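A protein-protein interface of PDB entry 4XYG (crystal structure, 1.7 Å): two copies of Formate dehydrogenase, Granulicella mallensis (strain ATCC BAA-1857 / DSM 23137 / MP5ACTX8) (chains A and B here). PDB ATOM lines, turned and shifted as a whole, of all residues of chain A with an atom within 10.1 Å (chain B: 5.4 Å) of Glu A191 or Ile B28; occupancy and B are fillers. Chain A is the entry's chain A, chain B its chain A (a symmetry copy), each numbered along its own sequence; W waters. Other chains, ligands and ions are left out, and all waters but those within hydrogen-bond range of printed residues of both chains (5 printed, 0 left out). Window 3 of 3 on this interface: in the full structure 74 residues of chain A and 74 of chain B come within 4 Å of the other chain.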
ATOM      1  N   ILE A 159      23.422  14.894  -7.549  1.00  0.00           N
ATOM      2  CA  ILE A 159      22.662  13.870  -8.267  1.00  0.00           C
ATOM      3  C   ILE A 159      22.074  12.842  -7.297  1.00  0.00           C
ATOM      4  O   ILE A 159      20.870  12.563  -7.335  1.00  0.00           O
ATOM      5  CB  ILE A 159      23.532  13.140  -9.307  1.00  0.00           C
ATOM      6  CG1 ILE A 159      23.911  14.106 -10.431  1.00  0.00           C
ATOM      7  CG2 ILE A 159      22.788  11.918  -9.867  1.00  0.00           C
ATOM      8  CD1 ILE A 159      24.952  13.552 -11.392  1.00  0.00           C
ATOM      9  N   LEU A 160      22.912  12.269  -6.442  1.00  0.00           N
ATOM     10  CA  LEU A 160      22.427  11.279  -5.477  1.00  0.00           C
ATOM     11  C   LEU A 160      21.363  11.871  -4.540  1.00  0.00           C
ATOM     12  O   LEU A 160      20.346  11.244  -4.269  1.00  0.00           O
ATOM     13  CB  LEU A 160      23.582  10.705  -4.654  1.00  0.00           C
ATOM     14  CG  LEU A 160      24.513   9.784  -5.442  1.00  0.00           C
ATOM     15  CD1 LEU A 160      25.819   9.621  -4.677  1.00  0.00           C
ATOM     16  CD2 LEU A 160      23.840   8.429  -5.654  1.00  0.00           C
ATOM     17  N   VAL A 163      17.906  12.272  -6.530  1.00  0.00           N
ATOM     18  CA  VAL A 163      17.249  11.027  -6.928  1.00  0.00           C
ATOM     19  C   VAL A 163      16.712  10.264  -5.706  1.00  0.00           C
ATOM     20  O   VAL A 163      15.604   9.710  -5.760  1.00  0.00           O
ATOM     21  CB  VAL A 163      18.184  10.164  -7.806  1.00  0.00           C
ATOM     22  CG1 VAL A 163      17.572   8.797  -8.087  1.00  0.00           C
ATOM     23  CG2 VAL A 163      18.481  10.888  -9.128  1.00  0.00           C
ATOM     24  N   ARG A 164      17.459  10.278  -4.602  1.00  0.00           N
ATOM     25  CA  ARG A 164      17.096   9.510  -3.396  1.00  0.00           C
ATOM     26  C   ARG A 164      16.179  10.264  -2.427  1.00  0.00           C
ATOM     27  O   ARG A 164      15.719   9.699  -1.435  1.00  0.00           O
ATOM     28  CB  ARG A 164      18.343   9.002  -2.658  1.00  0.00           C
ATOM     29  CG  ARG A 164      19.275   8.140  -3.511  1.00  0.00           C
ATOM     30  CD  ARG A 164      20.220   7.304  -2.638  1.00  0.00           C
ATOM     31  NE  ARG A 164      19.434   6.417  -1.779  1.00  0.00           N
ATOM     32  CZ  ARG A 164      18.913   5.254  -2.163  1.00  0.00           C
ATOM     33  NH1 ARG A 164      19.131   4.779  -3.383  1.00  0.00           N
ATOM     34  NH2 ARG A 164      18.166   4.567  -1.320  1.00  0.00           N
ATOM     35  N   SER A 187      11.643   8.676  -3.576  1.00  0.00           N
ATOM     36  CA  SER A 187      13.016   8.162  -3.426  1.00  0.00           C
ATOM     37  C   SER A 187      13.292   7.025  -4.400  1.00  0.00           C
ATOM     38  O   SER A 187      12.624   5.983  -4.353  1.00  0.00           O
ATOM     39  CB  SER A 187      13.256   7.702  -1.989  1.00  0.00           C
ATOM     40  OG  SER A 187      14.582   7.221  -1.805  1.00  0.00           O
ATOM     41  N   TYR A 188      14.275   7.226  -5.276  1.00  0.00           N
ATOM     42  CA  TYR A 188      14.650   6.223  -6.277  1.00  0.00           C
ATOM     43  C   TYR A 188      16.131   5.909  -6.135  1.00  0.00           C
ATOM     44  O   TYR A 188      16.882   6.701  -5.574  1.00  0.00           O
ATOM     45  CB  TYR A 188      14.392   6.745  -7.700  1.00  0.00           C
ATOM     46  CG  TYR A 188      12.941   7.056  -7.976  1.00  0.00           C
ATOM     47  CD1 TYR A 188      12.072   6.061  -8.390  1.00  0.00           C
ATOM     48  CD2 TYR A 188      12.448   8.342  -7.818  1.00  0.00           C
ATOM     49  CE1 TYR A 188      10.748   6.335  -8.640  1.00  0.00           C
ATOM     50  CE2 TYR A 188      11.109   8.631  -8.052  1.00  0.00           C
ATOM     51  CZ  TYR A 188      10.271   7.617  -8.468  1.00  0.00           C
ATOM     52  OH  TYR A 188       8.935   7.880  -8.714  1.00  0.00           O
ATOM     53  N   ASP A 189      16.545   4.762  -6.653  1.00  0.00           N
ATOM     54  CA  ASP A 189      17.962   4.451  -6.806  1.00  0.00           C
ATOM     55  C   ASP A 189      18.487   5.095  -8.090  1.00  0.00           C
ATOM     56  O   ASP A 189      17.753   5.258  -9.070  1.00  0.00           O
ATOM     57  CB  ASP A 189      18.188   2.941  -6.948  1.00  0.00           C
ATOM     58  CG  ASP A 189      17.834   2.151  -5.699  1.00  0.00           C
ATOM     59  OD1 ASP A 189      17.618   2.742  -4.619  1.00  0.00           O
ATOM     60  OD2 ASP A 189      17.793   0.898  -5.818  1.00  0.00           O
ATOM     61  N   LEU A 190      19.778   5.410  -8.098  1.00  0.00           N
ATOM     62  CA  LEU A 190      20.434   5.901  -9.299  1.00  0.00           C
ATOM     63  C   LEU A 190      20.742   4.754 -10.260  1.00  0.00           C
ATOM     64  O   LEU A 190      20.720   4.931 -11.481  1.00  0.00           O
ATOM     65  CB  LEU A 190      21.719   6.649  -8.913  1.00  0.00           C
ATOM     66  CG  LEU A 190      22.521   7.267 -10.053  1.00  0.00           C
ATOM     67  CD1 LEU A 190      21.694   8.308 -10.775  1.00  0.00           C
ATOM     68  CD2 LEU A 190      23.786   7.894  -9.479  1.00  0.00           C
ATOM     69  N   GLU A 191      21.013   3.572  -9.701  1.00  0.00           N
ATOM     70  CA  GLU A 191      21.384   2.386 -10.474  1.00  0.00           C
ATOM     71  C   GLU A 191      20.508   2.181 -11.714  1.00  0.00           C
ATOM     72  O   GLU A 191      19.279   2.217 -11.628  1.00  0.00           O
ATOM     73  CB  GLU A 191      21.321   1.129  -9.585  1.00  0.00           C
ATOM     74  CG  GLU A 191      21.943  -0.095 -10.238  1.00  0.00           C
ATOM     75  CD  GLU A 191      21.631  -1.388  -9.512  1.00  0.00           C
ATOM     76  OE1 GLU A 191      20.662  -1.431  -8.715  1.00  0.00           O
ATOM     77  OE2 GLU A 191      22.364  -2.369  -9.752  1.00  0.00           O
ATOM     78  N   GLY A 192      21.145   2.017 -12.868  1.00  0.00           N
ATOM     79  CA  GLY A 192      20.434   1.689 -14.095  1.00  0.00           C
ATOM     80  C   GLY A 192      19.846   2.873 -14.846  1.00  0.00           C
ATOM     81  O   GLY A 192      19.402   2.723 -15.985  1.00  0.00           O
ATOM     82  N   MET A 193      19.833   4.048 -14.223  1.00  0.00           N
ATOM     83  CA  MET A 193      19.371   5.240 -14.937  1.00  0.00           C
ATOM     84  C   MET A 193      20.311   5.610 -16.071  1.00  0.00           C
ATOM     85  O   MET A 193      21.495   5.254 -16.060  1.00  0.00           O
ATOM     86  CB  MET A 193      19.224   6.427 -13.988  1.00  0.00           C
ATOM     87  CG  MET A 193      18.072   6.296 -13.013  1.00  0.00           C
ATOM     88  SD  MET A 193      17.808   7.854 -12.167  1.00  0.00           S
ATOM     89  CE  MET A 193      16.287   7.470 -11.276  1.00  0.00           C
ATOM     90  N   HIS A 194      19.771   6.319 -17.058  1.00  0.00           N
ATOM     91  CA  HIS A 194      20.595   6.937 -18.089  1.00  0.00           C
ATOM     92  C   HIS A 194      21.055   8.309 -17.600  1.00  0.00           C
ATOM     93  O   HIS A 194      20.234   9.163 -17.280  1.00  0.00           O
ATOM     94  CB  HIS A 194      19.800   7.066 -19.395  1.00  0.00           C
ATOM     95  CG  HIS A 194      19.580   5.754 -20.085  1.00  0.00           C
ATOM     96  ND1 HIS A 194      20.364   5.323 -21.133  1.00  0.00           N
ATOM     97  CD2 HIS A 194      18.669   4.771 -19.870  1.00  0.00           C
ATOM     98  CE1 HIS A 194      19.951   4.132 -21.534  1.00  0.00           C
ATOM     99  NE2 HIS A 194      18.924   3.774 -20.783  1.00  0.00           N
ATOM    100  N   VAL A 195      22.373   8.512 -17.542  1.00  0.00           N
ATOM    101  CA  VAL A 195      22.930   9.769 -17.033  1.00  0.00           C
ATOM    102  C   VAL A 195      23.889  10.344 -18.062  1.00  0.00           C
ATOM    103  O   VAL A 195      24.748   9.632 -18.588  1.00  0.00           O
ATOM    104  CB  VAL A 195      23.671   9.576 -15.686  1.00  0.00           C
ATOM    105  CG1 VAL A 195      24.118  10.929 -15.138  1.00  0.00           C
ATOM    106  CG2 VAL A 195      22.766   8.878 -14.668  1.00  0.00           C
ATOM    107  N   LEU A 211      30.612   8.356 -11.732  1.00  0.00           N
ATOM    108  CA  LEU A 211      29.295   7.765 -11.950  1.00  0.00           C
ATOM    109  C   LEU A 211      29.378   6.305 -12.377  1.00  0.00           C
ATOM    110  O   LEU A 211      28.461   5.523 -12.096  1.00  0.00           O
ATOM    111  CB  LEU A 211      28.529   8.544 -13.020  1.00  0.00           C
ATOM    112  CG  LEU A 211      28.003   9.916 -12.608  1.00  0.00           C
ATOM    113  CD1 LEU A 211      27.474  10.682 -13.831  1.00  0.00           C
ATOM    114  CD2 LEU A 211      26.925   9.771 -11.534  1.00  0.00           C
ATOM    115  N   LYS A 212      30.452   5.939 -13.074  1.00  0.00           N
ATOM    116  CA  LYS A 212      30.536   4.607 -13.691  1.00  0.00           C
ATOM    117  C   LYS A 212      30.193   3.419 -12.752  1.00  0.00           C
ATOM    118  O   LYS A 212      29.382   2.565 -13.130  1.00  0.00           O
ATOM    119  CB  LYS A 212      31.883   4.379 -14.399  1.00  0.00           C
ATOM    120  CG  LYS A 212      31.935   3.027 -15.159  1.00  0.00           C
ATOM    121  CD  LYS A 212      33.229   2.817 -15.928  1.00  0.00           C
ATOM    122  CE  LYS A 212      33.222   1.468 -16.646  1.00  0.00           C
ATOM    123  NZ  LYS A 212      33.198   0.352 -15.659  1.00  0.00           N
ATOM    124  N   PRO A 213      30.787   3.359 -11.539  1.00  0.00           N
ATOM    125  CA  PRO A 213      30.496   2.190 -10.684  1.00  0.00           C
ATOM    126  C   PRO A 213      29.106   2.186 -10.057  1.00  0.00           C
ATOM    127  O   PRO A 213      28.771   1.209  -9.363  1.00  0.00           O
ATOM    128  CB  PRO A 213      31.565   2.277  -9.587  1.00  0.00           C
ATOM    129  CG  PRO A 213      31.856   3.753  -9.497  1.00  0.00           C
ATOM    130  CD  PRO A 213      31.805   4.234 -10.930  1.00  0.00           C
ATOM    131  N   PHE A 214      28.325   3.240 -10.275  1.00  0.00           N
ATOM    132  CA  PHE A 214      26.913   3.218  -9.857  1.00  0.00           C
ATOM    133  C   PHE A 214      26.043   2.416 -10.837  1.00  0.00           C
ATOM    134  O   PHE A 214      24.834   2.266 -10.629  1.00  0.00           O
ATOM    135  CB  PHE A 214      26.369   4.648  -9.656  1.00  0.00           C
ATOM    136  CG  PHE A 214      26.928   5.344  -8.440  1.00  0.00           C
ATOM    137  CD1 PHE A 214      26.236   5.323  -7.233  1.00  0.00           C
ATOM    138  CD2 PHE A 214      28.144   6.037  -8.508  1.00  0.00           C
ATOM    139  CE1 PHE A 214      26.758   5.957  -6.103  1.00  0.00           C
ATOM    140  CE2 PHE A 214      28.661   6.673  -7.385  1.00  0.00           C
ATOM    141  CZ  PHE A 214      27.970   6.638  -6.185  1.00  0.00           C
ATOM    142  N   ASP A 215      26.668   1.893 -11.892  1.00  0.00           N
ATOM    143  CA  ASP A 215      25.998   1.046 -12.889  1.00  0.00           C
ATOM    144  C   ASP A 215      24.879   1.784 -13.602  1.00  0.00           C
ATOM    145  O   ASP A 215      23.808   1.233 -13.877  1.00  0.00           O
ATOM    146  CB  ASP A 215      25.528  -0.295 -12.282  1.00  0.00           C
ATOM    147  CG  ASP A 215      26.675  -1.267 -12.067  1.00  0.00           C
ATOM    148  OD1 ASP A 215      27.713  -1.110 -12.739  1.00  0.00           O
ATOM    149  OD2 ASP A 215      26.543  -2.188 -11.227  1.00  0.00           O
ATOM    150  N   VAL A 216      25.152   3.047 -13.918  1.00  0.00           N
ATOM    151  CA  VAL A 216      24.278   3.818 -14.787  1.00  0.00           C
ATOM    152  C   VAL A 216      24.702   3.616 -16.235  1.00  0.00           C
ATOM    153  O   VAL A 216      25.797   3.112 -16.507  1.00  0.00           O
ATOM    154  CB  VAL A 216      24.331   5.310 -14.422  1.00  0.00           C
ATOM    155  CG1 VAL A 216      23.713   5.536 -13.050  1.00  0.00           C
ATOM    156  CG2 VAL A 216      25.767   5.811 -14.425  1.00  0.00           C
ATOM    157  N   LYS A 217      23.827   3.983 -17.164  1.00  0.00           N
ATOM    158  CA  LYS A 217      24.180   3.988 -18.580  1.00  0.00           C
ATOM    159  C   LYS A 217      24.627   5.405 -18.919  1.00  0.00           C
ATOM    160  O   LYS A 217      23.871   6.361 -18.724  1.00  0.00           O
ATOM    161  CB  LYS A 217      22.976   3.586 -19.444  1.00  0.00           C
ATOM    162  CG  LYS A 217      22.157   2.410 -18.903  1.00  0.00           C
ATOM    163  CD  LYS A 217      22.886   1.081 -18.984  1.00  0.00           C
ATOM    164  CE  LYS A 217      21.962  -0.052 -18.506  1.00  0.00           C
ATOM    165  NZ  LYS A 217      20.518   0.317 -18.677  1.00  0.00           N
ATOM    166  N   LEU A 218      25.862   5.544 -19.401  1.00  0.00           N
ATOM    167  CA  LEU A 218      26.504   6.859 -19.511  1.00  0.00           C
ATOM    168  C   LEU A 218      26.428   7.458 -20.911  1.00  0.00           C
ATOM    169  O   LEU A 218      26.668   6.771 -21.917  1.00  0.00           O
ATOM    170  CB  LEU A 218      27.982   6.766 -19.099  1.00  0.00           C
ATOM    171  CG  LEU A 218      28.286   6.492 -17.620  1.00  0.00           C
ATOM    172  CD1 LEU A 218      29.797   6.357 -17.394  1.00  0.00           C
ATOM    173  CD2 LEU A 218      27.712   7.593 -16.749  1.00  0.00           C
ATOM    174  N   ASP A 250      17.787  10.217 -17.995  1.00  0.00           N
ATOM    175  CA  ASP A 250      17.012  10.454 -16.783  1.00  0.00           C
ATOM    176  C   ASP A 250      17.623  11.578 -15.963  1.00  0.00           C
ATOM    177  O   ASP A 250      16.926  12.287 -15.227  1.00  0.00           O
ATOM    178  CB  ASP A 250      16.987   9.177 -15.935  1.00  0.00           C
ATOM    179  CG  ASP A 250      16.311   8.026 -16.651  1.00  0.00           C
ATOM    180  OD1 ASP A 250      15.104   8.164 -16.944  1.00  0.00           O
ATOM    181  OD2 ASP A 250      16.981   7.004 -16.935  1.00  0.00           O
ATOM    182  N   VAL A 251      18.943  11.710 -16.061  1.00  0.00           N
ATOM    183  CA  VAL A 251      19.679  12.704 -15.295  1.00  0.00           C
ATOM    184  C   VAL A 251      20.687  13.332 -16.242  1.00  0.00           C
ATOM    185  O   VAL A 251      21.372  12.615 -16.972  1.00  0.00           O
ATOM    186  CB  VAL A 251      20.481  12.042 -14.146  1.00  0.00           C
ATOM    187  CG1 VAL A 251      21.372  13.065 -13.457  1.00  0.00           C
ATOM    188  CG2 VAL A 251      19.543  11.376 -13.120  1.00  0.00           C
ATOM    189  N   PRO B  26      14.191   2.042 -13.928  1.00  0.00           N
ATOM    190  CA  PRO B  26      15.067   1.110 -14.651  1.00  0.00           C
ATOM    191  C   PRO B  26      14.732  -0.354 -14.378  1.00  0.00           C
ATOM    192  O   PRO B  26      14.326  -0.697 -13.267  1.00  0.00           O
ATOM    193  CB  PRO B  26      16.450   1.441 -14.085  1.00  0.00           C
ATOM    194  CG  PRO B  26      16.370   2.905 -13.768  1.00  0.00           C
ATOM    195  CD  PRO B  26      14.966   3.076 -13.210  1.00  0.00           C
ATOM    196  N   LYS B  27      14.897  -1.205 -15.383  1.00  0.00           N
ATOM    197  CA  LYS B  27      14.717  -2.637 -15.183  1.00  0.00           C
ATOM    198  C   LYS B  27      16.063  -3.243 -14.801  1.00  0.00           C
ATOM    199  O   LYS B  27      16.970  -3.321 -15.626  1.00  0.00           O
ATOM    200  CB  LYS B  27      14.182  -3.279 -16.465  1.00  0.00           C
ATOM    201  CG  LYS B  27      13.646  -4.698 -16.301  1.00  0.00           C
ATOM    202  CD  LYS B  27      13.138  -5.249 -17.637  1.00  0.00           C
ATOM    203  CE  LYS B  27      11.835  -4.584 -18.076  1.00  0.00           C
ATOM    204  NZ  LYS B  27      10.694  -5.549 -17.991  1.00  0.00           N
ATOM    205  N   ILE B  28      16.207  -3.645 -13.543  1.00  0.00           N
ATOM    206  CA  ILE B  28      17.437  -4.294 -13.090  1.00  0.00           C
ATOM    207  C   ILE B  28      17.278  -5.796 -13.343  1.00  0.00           C
ATOM    208  O   ILE B  28      16.221  -6.359 -13.058  1.00  0.00           O
ATOM    209  CB  ILE B  28      17.710  -3.997 -11.591  1.00  0.00           C
ATOM    210  CG1 ILE B  28      17.742  -2.480 -11.343  1.00  0.00           C
ATOM    211  CG2 ILE B  28      19.008  -4.664 -11.124  1.00  0.00           C
ATOM    212  CD1 ILE B  28      18.765  -1.723 -12.217  1.00  0.00           C
ATOM    213  N   GLU B  29      18.309  -6.431 -13.897  1.00  0.00           N
ATOM    214  CA  GLU B  29      18.234  -7.844 -14.279  1.00  0.00           C
ATOM    215  C   GLU B  29      19.009  -8.760 -13.345  1.00  0.00           C
ATOM    216  O   GLU B  29      18.612  -9.903 -13.094  1.00  0.00           O
ATOM    217  CB  GLU B  29      18.784  -8.044 -15.686  1.00  0.00           C
ATOM    218  CG  GLU B  29      17.995  -7.363 -16.772  1.00  0.00           C
ATOM    219  CD  GLU B  29      17.890  -8.221 -18.014  1.00  0.00           C
ATOM    220  OE1 GLU B  29      18.870  -8.930 -18.333  1.00  0.00           O
ATOM    221  OE2 GLU B  29      16.821  -8.193 -18.664  1.00  0.00           O
ATOM    222  N   ARG B  30      20.142  -8.273 -12.857  1.00  0.00           N
ATOM    223  CA  ARG B  30      20.944  -9.083 -11.955  1.00  0.00           C
ATOM    224  C   ARG B  30      21.735  -8.230 -10.985  1.00  0.00           C
ATOM    225  O   ARG B  30      21.873  -7.021 -11.175  1.00  0.00           O
ATOM    226  CB  ARG B  30      21.868  -9.998 -12.748  1.00  0.00           C
ATOM    227  CG  ARG B  30      22.952  -9.268 -13.478  1.00  0.00           C
ATOM    228  CD  ARG B  30      23.435 -10.088 -14.661  1.00  0.00           C
ATOM    229  NE  ARG B  30      22.393 -10.172 -15.677  1.00  0.00           N
ATOM    230  CZ  ARG B  30      22.614 -10.401 -16.968  1.00  0.00           C
ATOM    231  NH1 ARG B  30      23.853 -10.582 -17.410  1.00  0.00           N
ATOM    232  NH2 ARG B  30      21.594 -10.451 -17.815  1.00  0.00           N
ATOM    233  N   TYR B  31      22.246  -8.876  -9.945  1.00  0.00           N
ATOM    234  CA  TYR B  31      23.032  -8.220  -8.916  1.00  0.00           C
ATOM    235  C   TYR B  31      24.504  -8.398  -9.262  1.00  0.00           C
ATOM    236  O   TYR B  31      24.829  -9.194 -10.149  1.00  0.00           O
ATOM    237  CB  TYR B  31      22.692  -8.847  -7.562  1.00  0.00           C
ATOM    238  CG  TYR B  31      21.231  -8.690  -7.192  1.00  0.00           C
ATOM    239  CD1 TYR B  31      20.666  -7.434  -7.055  1.00  0.00           C
ATOM    240  CD2 TYR B  31      20.418  -9.801  -6.977  1.00  0.00           C
ATOM    241  CE1 TYR B  31      19.330  -7.269  -6.709  1.00  0.00           C
ATOM    242  CE2 TYR B  31      19.064  -9.645  -6.640  1.00  0.00           C
ATOM    243  CZ  TYR B  31      18.538  -8.372  -6.517  1.00  0.00           C
ATOM    244  OH  TYR B  31      17.211  -8.180  -6.165  1.00  0.00           O
ATOM    245  N   VAL B  37      17.636 -11.128 -10.281  1.00  0.00           N
ATOM    246  CA  VAL B  37      16.538 -10.470  -9.573  1.00  0.00           C
ATOM    247  C   VAL B  37      15.358 -11.431  -9.477  1.00  0.00           C
ATOM    248  O   VAL B  37      15.344 -12.451 -10.166  1.00  0.00           O
ATOM    249  CB  VAL B  37      16.096  -9.169 -10.268  1.00  0.00           C
ATOM    250  CG1 VAL B  37      17.253  -8.163 -10.299  1.00  0.00           C
ATOM    251  CG2 VAL B  37      15.560  -9.453 -11.670  1.00  0.00           C
ATOM    252  N   ILE B 149      21.910  -2.563  -3.065  1.00  0.00           N
ATOM    253  CA  ILE B 149      22.441  -1.422  -3.824  1.00  0.00           C
ATOM    254  C   ILE B 149      21.854  -0.097  -3.317  1.00  0.00           C
ATOM    255  O   ILE B 149      22.563   0.920  -3.268  1.00  0.00           O
ATOM    256  CB  ILE B 149      22.230  -1.573  -5.346  1.00  0.00           C
ATOM    257  CG1 ILE B 149      22.967  -2.814  -5.888  1.00  0.00           C
ATOM    258  CG2 ILE B 149      22.678  -0.283  -6.085  1.00  0.00           C
ATOM    259  CD1 ILE B 149      24.463  -2.892  -5.547  1.00  0.00           C
ATOM    260  N   GLU B 153      24.165   3.148  -2.126  1.00  0.00           N
ATOM    261  CA  GLU B 153      24.006   4.505  -2.645  1.00  0.00           C
ATOM    262  C   GLU B 153      23.743   5.514  -1.543  1.00  0.00           C
ATOM    263  O   GLU B 153      24.314   6.601  -1.548  1.00  0.00           O
ATOM    264  CB  GLU B 153      22.863   4.581  -3.659  1.00  0.00           C
ATOM    265  CG  GLU B 153      23.106   3.832  -4.964  1.00  0.00           C
ATOM    266  CD  GLU B 153      21.972   4.058  -5.944  1.00  0.00           C
ATOM    267  OE1 GLU B 153      21.102   4.907  -5.646  1.00  0.00           O
ATOM    268  OE2 GLU B 153      21.960   3.418  -7.015  1.00  0.00           O
ATOM    269  N   ARG B 210      31.939   1.939  -5.437  1.00  0.00           N
ATOM    270  CA  ARG B 210      31.466   3.292  -5.736  1.00  0.00           C
ATOM    271  C   ARG B 210      32.437   4.367  -5.250  1.00  0.00           C
ATOM    272  O   ARG B 210      32.547   5.446  -5.855  1.00  0.00           O
ATOM    273  CB  ARG B 210      30.040   3.486  -5.163  1.00  0.00           C
ATOM    274  CG  ARG B 210      28.991   2.781  -6.027  1.00  0.00           C
ATOM    275  CD  ARG B 210      27.681   2.485  -5.302  1.00  0.00           C
ATOM    276  NE  ARG B 210      26.741   1.837  -6.236  1.00  0.00           N
ATOM    277  CZ  ARG B 210      26.854   0.591  -6.694  1.00  0.00           C
ATOM    278  NH1 ARG B 210      27.863  -0.202  -6.317  1.00  0.00           N
ATOM    279  NH2 ARG B 210      25.950   0.136  -7.557  1.00  0.00           N
ATOM    280  N   ARG B 344      11.741  -4.629  -6.287  1.00  0.00           N
ATOM    281  CA  ARG B 344      12.405  -5.925  -6.224  1.00  0.00           C
ATOM    282  C   ARG B 344      11.957  -6.778  -5.040  1.00  0.00           C
ATOM    283  O   ARG B 344      11.700  -7.972  -5.202  1.00  0.00           O
ATOM    284  CB  ARG B 344      13.931  -5.760  -6.221  1.00  0.00           C
ATOM    285  CG  ARG B 344      14.424  -5.140  -7.518  1.00  0.00           C
ATOM    286  CD  ARG B 344      15.949  -5.126  -7.573  1.00  0.00           C
ATOM    287  NE  ARG B 344      16.572  -4.279  -6.551  1.00  0.00           N
ATOM    288  CZ  ARG B 344      16.881  -2.992  -6.714  1.00  0.00           C
ATOM    289  NH1 ARG B 344      16.586  -2.370  -7.850  1.00  0.00           N
ATOM    290  NH2 ARG B 344      17.478  -2.314  -5.733  1.00  0.00           N
HETATM  291  O   HOH W   1      20.042  -3.909  -7.460  1.00  0.00           O
HETATM  292  O   HOH W   2      25.238  -2.275  -9.115  1.00  0.00           O
HETATM  293  O   HOH W   3      21.996  -4.854  -9.037  1.00  0.00           O
HETATM  294  O   HOH W   4      18.382  -0.163  -8.129  1.00  0.00           O
HETATM  295  O   HOH W   5      24.341   2.425  -7.938  1.00  0.00           O
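The guanidinium group (NH1) of Arg A164 lies within salt-bridge range of the side-chain carboxylate (OE1) of Glu B153 (3.0 Å). NH2 of Arg B344 is in salt-bridge range of OD2 of Asp A189 (3.2 Å). OE1 of Glu B153 is in hydrogen-bond range of N of Leu A190. The side-chain carboxylate (OE2) of Glu B153 is in hydrogen-bond range of the backbone NH (N) of Glu A191 (2.9 Å). The backbone carbonyl oxygen (O) of Pro A213 lies close to the guanidinium group (NH1) of Arg B210.
O of Arg A164 sits at hydrogen-bond distance from OG of Ser A187, 2.8 Å away. The side-chain carboxylate (OD1) of Asp A189 lies within salt-bridge range of the guanidinium group (NH1) of Arg A164. The backbone NH (N) of Gly A192 lies within hydrogen-bond range of the backbone carbonyl oxygen (O) of Asp A215, 3.0 Å away. O of Met A193 lies within hydrogen-bond range of N of Lys A217.
Among the printed residues, pairs that only touch across the chains: Asp A189 with Glu B153 (3.4 Å), Glu A191 with Pro B26 (3.7 Å), Glu A191 with Ile B28 (3.96 Å), Glu A191 with Ile B149 (3.5 Å), Gly A192 with Pro B26 (3.6 Å), Met A193 with Pro B26 (3.7 Å) and Phe A214 with Arg B210 (3.7 Å).
Of the 23 printed residues of chain A, 8 touch a printed residue of chain B. Hydrophobic or aromatic side chains of chain A that line the printed part of chain B: Leu A190, Met A193, Pro A213 and Phe A214. Among the printed residues, 12 pairs touch across the chains.
Water W2 lies within hydrogen-bond range of OD2 of Asp A215 (2.5 Å), OE2 of Glu A191 (2.9 Å) and NH2 of Arg B210 (3.0 Å). Water W4 lies within hydrogen-bond range of OD2 of Asp A189, OE1 of Glu A191 and NH1 of Arg B344. Water W3 bridges OE2 of Glu A191 (2.6 Å) and O of Arg B30 (3.0 Å). Water W5 lies within hydrogen-bond range of the side-chain carboxylate (OE2) of Glu B153, the backbone carbonyl oxygen (O) of Phe A214 and the guanidinium group (NH2) of Arg B210. Water W1 lies within hydrogen-bond range of OE1 of Glu A191 (2.8 Å) and NH2 of Arg B344 (3.5 Å).
No position is printed for both chains. Of the 12 pairs that touch across the chains among the printed residues, none has its exchanged pair printed and touching as well.
Printed residues of chain B within 4 Å of Glu A191: Pro B26 (3.7 Å), Ile B28 (3.96 Å), Ile B149 (3.5 Å) and Glu B153 (2.9 Å). Of the printed residues of chain B, Met A193 touches Pro B26 (3.7 Å). Of the printed residues of chain A, Ile B28 touches Glu A191 (3.96 Å). Printed residues of chain A within 4 Å of Glu B153: Arg A164 (3.0 Å), Asp A189 (3.4 Å), Leu A190 (2.8 Å) and Glu A191 (2.9 Å). Of the printed residues of chain A, Arg B210 touches Pro A213 (3.3 Å) and Phe A214 (3.7 Å).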
